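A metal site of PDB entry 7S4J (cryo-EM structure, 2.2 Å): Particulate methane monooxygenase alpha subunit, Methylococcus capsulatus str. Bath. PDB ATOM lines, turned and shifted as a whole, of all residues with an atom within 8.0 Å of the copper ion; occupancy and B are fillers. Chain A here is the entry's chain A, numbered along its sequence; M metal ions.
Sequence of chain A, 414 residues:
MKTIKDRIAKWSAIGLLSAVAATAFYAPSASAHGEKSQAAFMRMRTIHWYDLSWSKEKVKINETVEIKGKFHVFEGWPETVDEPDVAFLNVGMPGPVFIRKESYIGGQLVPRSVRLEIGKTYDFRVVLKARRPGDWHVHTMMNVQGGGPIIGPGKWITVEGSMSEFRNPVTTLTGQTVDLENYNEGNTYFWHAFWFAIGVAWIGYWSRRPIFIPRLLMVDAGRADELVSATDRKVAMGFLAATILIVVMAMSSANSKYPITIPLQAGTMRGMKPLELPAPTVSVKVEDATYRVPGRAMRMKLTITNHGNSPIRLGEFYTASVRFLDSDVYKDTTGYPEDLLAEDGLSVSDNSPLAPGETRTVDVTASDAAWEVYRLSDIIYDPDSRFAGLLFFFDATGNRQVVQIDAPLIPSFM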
ATOM      1  N   MET A  44      -5.749  -7.785  -7.531  1.00  0.00           N
ATOM      2  CA  MET A  44      -5.551  -6.396  -7.943  1.00  0.00           C
ATOM      3  C   MET A  44      -4.466  -5.708  -7.140  1.00  0.00           C
ATOM      4  O   MET A  44      -3.698  -4.912  -7.689  1.00  0.00           O
ATOM      5  CB  MET A  44      -6.856  -5.620  -7.836  1.00  0.00           C
ATOM      6  CG  MET A  44      -7.798  -5.807  -9.013  1.00  0.00           C
ATOM      7  SD  MET A  44      -9.495  -5.364  -8.590  1.00  0.00           S
ATOM      8  CE  MET A  44     -10.249  -5.356 -10.202  1.00  0.00           C
ATOM      9  N   ARG A  45      -4.385  -5.968  -5.832  1.00  0.00           N
ATOM     10  CA  ARG A  45      -3.379  -5.337  -4.999  1.00  0.00           C
ATOM     11  C   ARG A  45      -2.491  -6.386  -4.320  1.00  0.00           C
ATOM     12  O   ARG A  45      -2.559  -6.574  -3.113  1.00  0.00           O
ATOM     13  CB  ARG A  45      -4.058  -4.482  -3.939  1.00  0.00           C
ATOM     14  CG  ARG A  45      -5.426  -3.905  -4.267  1.00  0.00           C
ATOM     15  CD  ARG A  45      -6.280  -3.836  -3.006  1.00  0.00           C
ATOM     16  NE  ARG A  45      -5.893  -2.732  -2.129  1.00  0.00           N
ATOM     17  CZ  ARG A  45      -6.190  -1.460  -2.319  1.00  0.00           C
ATOM     18  NH1 ARG A  45      -6.877  -1.056  -3.370  1.00  0.00           N
ATOM     19  NH2 ARG A  45      -5.789  -0.570  -1.414  1.00  0.00           N
ATOM     20  N   THR A  46      -1.616  -7.027  -5.092  1.00  0.00           N
ATOM     21  CA  THR A  46      -0.441  -7.635  -4.498  1.00  0.00           C
ATOM     22  C   THR A  46       0.813  -7.256  -5.250  1.00  0.00           C
ATOM     23  O   THR A  46       1.725  -6.614  -4.708  1.00  0.00           O
ATOM     24  CB  THR A  46      -0.590  -9.157  -4.429  1.00  0.00           C
ATOM     25  OG1 THR A  46      -1.507  -9.599  -5.444  1.00  0.00           O
ATOM     26  CG2 THR A  46      -1.102  -9.573  -3.065  1.00  0.00           C
ATOM     27  N   ILE A  47       0.852  -7.608  -6.531  1.00  0.00           N
ATOM     28  CA  ILE A  47       2.043  -7.488  -7.371  1.00  0.00           C
ATOM     29  C   ILE A  47       1.571  -7.204  -8.777  1.00  0.00           C
ATOM     30  O   ILE A  47       0.715  -7.916  -9.309  1.00  0.00           O
ATOM     31  CB  ILE A  47       2.912  -8.755  -7.339  1.00  0.00           C
ATOM     32  CG1 ILE A  47       3.758  -8.804  -6.066  1.00  0.00           C
ATOM     33  CG2 ILE A  47       3.826  -8.809  -8.548  1.00  0.00           C
ATOM     34  CD1 ILE A  47       4.461 -10.107  -5.864  1.00  0.00           C
ATOM     35  N   HIS A  48       2.125  -6.176  -9.397  1.00  0.00           N
ATOM     36  CA  HIS A  48       1.754  -5.770 -10.747  1.00  0.00           C
ATOM     37  C   HIS A  48       2.878  -6.144 -11.699  1.00  0.00           C
ATOM     38  O   HIS A  48       3.974  -5.586 -11.625  1.00  0.00           O
ATOM     39  CB  HIS A  48       1.478  -4.271 -10.788  1.00  0.00           C
ATOM     40  CG  HIS A  48       0.442  -3.818  -9.805  1.00  0.00           C
ATOM     41  ND1 HIS A  48       0.539  -2.640  -9.116  1.00  0.00           N
ATOM     42  CD2 HIS A  48      -0.718  -4.395  -9.403  1.00  0.00           C
ATOM     43  CE1 HIS A  48      -0.508  -2.504  -8.321  1.00  0.00           C
ATOM     44  NE2 HIS A  48      -1.287  -3.557  -8.479  1.00  0.00           N
ATOM     45  N   TRP A  49       2.608  -7.084 -12.587  1.00  0.00           N
ATOM     46  CA  TRP A  49       3.574  -7.527 -13.587  1.00  0.00           C
ATOM     47  C   TRP A  49       3.381  -6.705 -14.855  1.00  0.00           C
ATOM     48  O   TRP A  49       2.270  -6.628 -15.389  1.00  0.00           O
ATOM     49  CB  TRP A  49       3.407  -9.013 -13.899  1.00  0.00           C
ATOM     50  CG  TRP A  49       3.276  -9.887 -12.700  1.00  0.00           C
ATOM     51  CD1 TRP A  49       2.150 -10.093 -11.955  1.00  0.00           C
ATOM     52  CD2 TRP A  49       4.297 -10.701 -12.112  1.00  0.00           C
ATOM     53  NE1 TRP A  49       2.410 -10.970 -10.945  1.00  0.00           N
ATOM     54  CE2 TRP A  49       3.718 -11.367 -11.017  1.00  0.00           C
ATOM     55  CE3 TRP A  49       5.641 -10.923 -12.412  1.00  0.00           C
ATOM     56  CZ2 TRP A  49       4.441 -12.241 -10.212  1.00  0.00           C
ATOM     57  CZ3 TRP A  49       6.352 -11.793 -11.608  1.00  0.00           C
ATOM     58  CH2 TRP A  49       5.751 -12.440 -10.523  1.00  0.00           C
ATOM     59  N   TYR A  50       4.457  -6.097 -15.332  1.00  0.00           N
ATOM     60  CA  TYR A  50       4.407  -5.353 -16.576  1.00  0.00           C
ATOM     61  C   TYR A  50       5.756  -5.442 -17.265  1.00  0.00           C
ATOM     62  O   TYR A  50       6.742  -5.916 -16.698  1.00  0.00           O
ATOM     63  CB  TYR A  50       3.982  -3.892 -16.351  1.00  0.00           C
ATOM     64  CG  TYR A  50       4.969  -3.038 -15.599  1.00  0.00           C
ATOM     65  CD1 TYR A  50       5.066  -3.113 -14.216  1.00  0.00           C
ATOM     66  CD2 TYR A  50       5.796  -2.148 -16.260  1.00  0.00           C
ATOM     67  CE1 TYR A  50       5.959  -2.329 -13.531  1.00  0.00           C
ATOM     68  CE2 TYR A  50       6.692  -1.364 -15.593  1.00  0.00           C
ATOM     69  CZ  TYR A  50       6.771  -1.448 -14.219  1.00  0.00           C
ATOM     70  OH  TYR A  50       7.671  -0.671 -13.540  1.00  0.00           O
ATOM     71  N   PHE A  71       8.140  -6.477 -11.994  1.00  0.00           N
ATOM     72  CA  PHE A  71       7.002  -6.540 -11.100  1.00  0.00           C
ATOM     73  C   PHE A  71       7.146  -5.480 -10.019  1.00  0.00           C
ATOM     74  O   PHE A  71       8.254  -5.240  -9.520  1.00  0.00           O
ATOM     75  CB  PHE A  71       6.808  -7.945 -10.478  1.00  0.00           C
ATOM     76  CG  PHE A  71       7.917  -8.370  -9.559  1.00  0.00           C
ATOM     77  CD1 PHE A  71       7.862  -8.089  -8.198  1.00  0.00           C
ATOM     78  CD2 PHE A  71       8.994  -9.097 -10.040  1.00  0.00           C
ATOM     79  CE1 PHE A  71       8.859  -8.495  -7.354  1.00  0.00           C
ATOM     80  CE2 PHE A  71       9.998  -9.502  -9.189  1.00  0.00           C
ATOM     81  CZ  PHE A  71       9.931  -9.201  -7.847  1.00  0.00           C
ATOM     82  N   HIS A  72       6.042  -4.837  -9.683  1.00  0.00           N
ATOM     83  CA  HIS A  72       5.997  -3.829  -8.649  1.00  0.00           C
ATOM     84  C   HIS A  72       5.219  -4.382  -7.456  1.00  0.00           C
ATOM     85  O   HIS A  72       4.121  -4.900  -7.633  1.00  0.00           O
ATOM     86  CB  HIS A  72       5.352  -2.545  -9.159  1.00  0.00           C
ATOM     87  CG  HIS A  72       5.122  -1.527  -8.084  1.00  0.00           C
ATOM     88  ND1 HIS A  72       3.855  -1.130  -7.699  1.00  0.00           N
ATOM     89  CD2 HIS A  72       5.980  -0.826  -7.311  1.00  0.00           C
ATOM     90  CE1 HIS A  72       3.955  -0.230  -6.737  1.00  0.00           C
ATOM     91  NE2 HIS A  72       5.230  -0.036  -6.485  1.00  0.00           N
ATOM     92  N   VAL A  73       5.808  -4.277  -6.273  1.00  0.00           N
ATOM     93  CA  VAL A  73       5.130  -4.700  -5.054  1.00  0.00           C
ATOM     94  C   VAL A  73       4.223  -3.555  -4.596  1.00  0.00           C
ATOM     95  O   VAL A  73       4.701  -2.451  -4.332  1.00  0.00           O
ATOM     96  CB  VAL A  73       6.137  -5.093  -3.967  1.00  0.00           C
ATOM     97  CG1 VAL A  73       5.422  -5.701  -2.774  1.00  0.00           C
ATOM     98  CG2 VAL A  73       7.150  -6.072  -4.524  1.00  0.00           C
ATOM     99  N   PHE A  74       2.925  -3.825  -4.506  1.00  0.00           N
ATOM    100  CA  PHE A  74       1.970  -2.767  -4.216  1.00  0.00           C
ATOM    101  C   PHE A  74       2.142  -2.234  -2.799  1.00  0.00           C
ATOM    102  O   PHE A  74       2.329  -3.005  -1.857  1.00  0.00           O
ATOM    103  CB  PHE A  74       0.551  -3.274  -4.415  1.00  0.00           C
ATOM    104  CG  PHE A  74      -0.495  -2.219  -4.245  1.00  0.00           C
ATOM    105  CD1 PHE A  74      -0.400  -1.016  -4.927  1.00  0.00           C
ATOM    106  CD2 PHE A  74      -1.558  -2.397  -3.382  1.00  0.00           C
ATOM    107  CE1 PHE A  74      -1.345  -0.036  -4.764  1.00  0.00           C
ATOM    108  CE2 PHE A  74      -2.517  -1.420  -3.233  1.00  0.00           C
ATOM    109  CZ  PHE A  74      -2.410  -0.243  -3.910  1.00  0.00           C
ATOM    110  N   GLU A  75       2.059  -0.904  -2.657  1.00  0.00           N
ATOM    111  CA  GLU A  75       2.226  -0.281  -1.346  1.00  0.00           C
ATOM    112  C   GLU A  75       1.095  -0.669  -0.404  1.00  0.00           C
ATOM    113  O   GLU A  75       1.325  -0.899   0.795  1.00  0.00           O
ATOM    114  CB  GLU A  75       2.298   1.231  -1.493  1.00  0.00           C
ATOM    115  CG  GLU A  75       3.615   1.741  -2.056  1.00  0.00           C
ATOM    116  CD  GLU A  75       3.660   1.702  -3.565  1.00  0.00           C
ATOM    117  OE1 GLU A  75       2.674   1.244  -4.170  1.00  0.00           O
ATOM    118  OE2 GLU A  75       4.673   2.132  -4.141  1.00  0.00           O
ATOM    119  N   GLY A  76      -0.134  -0.728  -0.903  1.00  0.00           N
ATOM    120  CA  GLY A  76      -1.265  -1.139  -0.086  1.00  0.00           C
ATOM    121  C   GLY A  76      -1.394  -2.638   0.017  1.00  0.00           C
ATOM    122  O   GLY A  76      -2.459  -3.203  -0.257  1.00  0.00           O
ATOM    123  N   GLY A 119       6.469  -1.660  -2.084  1.00  0.00           N
ATOM    124  CA  GLY A 119       6.587  -0.401  -2.781  1.00  0.00           C
ATOM    125  C   GLY A 119       7.682  -0.346  -3.830  1.00  0.00           C
ATOM    126  O   GLY A 119       7.735   0.617  -4.595  1.00  0.00           O
ATOM    127  N   LYS A 120       8.542  -1.351  -3.892  1.00  0.00           N
ATOM    128  CA  LYS A 120       9.664  -1.361  -4.817  1.00  0.00           C
ATOM    129  C   LYS A 120       9.294  -2.070  -6.115  1.00  0.00           C
ATOM    130  O   LYS A 120       8.362  -2.873  -6.179  1.00  0.00           O
ATOM    131  CB  LYS A 120      10.879  -2.028  -4.186  1.00  0.00           C
ATOM    132  CG  LYS A 120      11.485  -1.258  -3.045  1.00  0.00           C
ATOM    133  CD  LYS A 120      12.190  -0.021  -3.572  1.00  0.00           C
ATOM    134  CE  LYS A 120      12.330   1.031  -2.486  1.00  0.00           C
ATOM    135  NZ  LYS A 120      13.317   2.073  -2.888  1.00  0.00           N
ATOM    136  N   THR A 121      10.058  -1.762  -7.163  1.00  0.00           N
ATOM    137  CA  THR A 121       9.907  -2.398  -8.461  1.00  0.00           C
ATOM    138  C   THR A 121      11.174  -3.186  -8.768  1.00  0.00           C
ATOM    139  O   THR A 121      12.287  -2.657  -8.623  1.00  0.00           O
ATOM    140  CB  THR A 121       9.662  -1.356  -9.563  1.00  0.00           C
ATOM    141  OG1 THR A 121       8.486  -0.609  -9.255  1.00  0.00           O
ATOM    142  CG2 THR A 121       9.487  -2.029 -10.902  1.00  0.00           C
ATOM    143  N   TYR A 318      -3.749  -1.203 -16.535  1.00  0.00           N
ATOM    144  CA  TYR A 318      -3.497  -2.572 -16.119  1.00  0.00           C
ATOM    145  C   TYR A 318      -4.027  -2.734 -14.698  1.00  0.00           C
ATOM    146  O   TYR A 318      -3.671  -1.952 -13.820  1.00  0.00           O
ATOM    147  CB  TYR A 318      -1.992  -2.871 -16.187  1.00  0.00           C
ATOM    148  CG  TYR A 318      -1.539  -4.104 -15.464  1.00  0.00           C
ATOM    149  CD1 TYR A 318      -1.266  -4.083 -14.098  1.00  0.00           C
ATOM    150  CD2 TYR A 318      -1.350  -5.305 -16.137  1.00  0.00           C
ATOM    151  CE1 TYR A 318      -0.849  -5.212 -13.438  1.00  0.00           C
ATOM    152  CE2 TYR A 318      -0.933  -6.434 -15.477  1.00  0.00           C
ATOM    153  CZ  TYR A 318      -0.682  -6.380 -14.136  1.00  0.00           C
ATOM    154  OH  TYR A 318      -0.258  -7.508 -13.468  1.00  0.00           O
ATOM    155  N   ALA A 388      -6.622  -1.766  -7.363  1.00  0.00           N
ATOM    156  CA  ALA A 388      -5.376  -1.080  -7.636  1.00  0.00           C
ATOM    157  C   ALA A 388      -4.944  -1.430  -9.051  1.00  0.00           C
ATOM    158  O   ALA A 388      -5.347  -2.459  -9.598  1.00  0.00           O
ATOM    159  CB  ALA A 388      -4.284  -1.462  -6.635  1.00  0.00           C
ATOM    160  N   GLY A 389      -4.142  -0.562  -9.643  1.00  0.00           N
ATOM    161  CA  GLY A 389      -3.700  -0.806 -10.996  1.00  0.00           C
ATOM    162  C   GLY A 389      -2.641   0.178 -11.419  1.00  0.00           C
ATOM    163  O   GLY A 389      -2.211   1.036 -10.652  1.00  0.00           O
ATOM    164  N   LEU A 390      -2.222   0.048 -12.680  1.00  0.00           N
ATOM    165  CA  LEU A 390      -1.194   0.890 -13.265  1.00  0.00           C
ATOM    166  C   LEU A 390      -1.757   1.602 -14.478  1.00  0.00           C
ATOM    167  O   LEU A 390      -2.414   0.982 -15.318  1.00  0.00           O
ATOM    168  CB  LEU A 390       0.034   0.070 -13.658  1.00  0.00           C
ATOM    169  CG  LEU A 390       0.754  -0.710 -12.564  1.00  0.00           C
ATOM    170  CD1 LEU A 390       1.904  -1.484 -13.154  1.00  0.00           C
ATOM    171  CD2 LEU A 390       1.248   0.231 -11.476  1.00  0.00           C
ATOM    172  N   VAL A 402       4.677   5.409 -15.785  1.00  0.00           N
ATOM    173  CA  VAL A 402       3.847   4.479 -15.044  1.00  0.00           C
ATOM    174  C   VAL A 402       3.398   5.156 -13.766  1.00  0.00           C
ATOM    175  O   VAL A 402       4.213   5.530 -12.925  1.00  0.00           O
ATOM    176  CB  VAL A 402       4.604   3.180 -14.728  1.00  0.00           C
ATOM    177  CG1 VAL A 402       3.665   2.152 -14.136  1.00  0.00           C
ATOM    178  CG2 VAL A 402       5.284   2.642 -15.970  1.00  0.00           C
ATOM    179  N   VAL A 403       2.086   5.311 -13.618  1.00  0.00           N
ATOM    180  CA  VAL A 403       1.519   5.841 -12.387  1.00  0.00           C
ATOM    181  C   VAL A 403       0.608   4.789 -11.792  1.00  0.00           C
ATOM    182  O   VAL A 403      -0.035   4.014 -12.500  1.00  0.00           O
ATOM    183  CB  VAL A 403       0.765   7.186 -12.600  1.00  0.00           C
ATOM    184  CG1 VAL A 403       1.570   8.118 -13.485  1.00  0.00           C
ATOM    185  CG2 VAL A 403      -0.597   6.950 -13.186  1.00  0.00           C
ATOM    186  N   GLN A 404       0.586   4.725 -10.463  1.00  0.00           N
ATOM    187  CA  GLN A 404      -0.182   3.728  -9.747  1.00  0.00           C
ATOM    188  C   GLN A 404      -1.403   4.373  -9.114  1.00  0.00           C
ATOM    189  O   GLN A 404      -1.305   5.455  -8.526  1.00  0.00           O
ATOM    190  CB  GLN A 404       0.658   3.055  -8.673  1.00  0.00           C
ATOM    191  CG  GLN A 404      -0.094   2.007  -7.882  1.00  0.00           C
ATOM    192  CD  GLN A 404       0.816   1.087  -7.114  1.00  0.00           C
ATOM    193  OE1 GLN A 404       1.083  -0.040  -7.534  1.00  0.00           O
ATOM    194  NE2 GLN A 404       1.314   1.559  -5.971  1.00  0.00           N
ATOM    195  N   ILE A 405      -2.549   3.716  -9.268  1.00  0.00           N
ATOM    196  CA  ILE A 405      -3.816   4.222  -8.740  1.00  0.00           C
ATOM    197  C   ILE A 405      -4.455   3.133  -7.886  1.00  0.00           C
ATOM    198  O   ILE A 405      -4.336   1.939  -8.195  1.00  0.00           O
ATOM    199  CB  ILE A 405      -4.778   4.660  -9.863  1.00  0.00           C
ATOM    200  CG1 ILE A 405      -5.031   3.512 -10.839  1.00  0.00           C
ATOM    201  CG2 ILE A 405      -4.204   5.855 -10.608  1.00  0.00           C
ATOM    202  CD1 ILE A 405      -6.178   3.773 -11.770  1.00  0.00           C
HETATM  203 CU    CU M   1       2.181  -2.001  -8.278  1.00  0.00          CU
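A ring nitrogen (NE2) of His 72 lies within hydrogen-bond range of the side-chain carboxylate (OE2) of Glu 75, at 3.2 Å. The backbone carbonyl oxygen of Gly 119 is in hydrogen-bond range of a ring nitrogen (NE2) of His 72 (3.2 Å). NE2 of His 48 lies within hydrogen-bond range of O of Met 44, at 2.9 Å.
The nearest printed residue that does not touch the copper ion is Leu 390 (4.01 Å).
The copper ion is bound by a ring nitrogen (ND1) of His 48 (2.0 Å), a ring nitrogen (ND1) of His 72 (2.0 Å) and the side-chain amide oxygen (OE1) of Gln 404 (2.4 Å). The copper ion has three donor atoms within binding distance.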
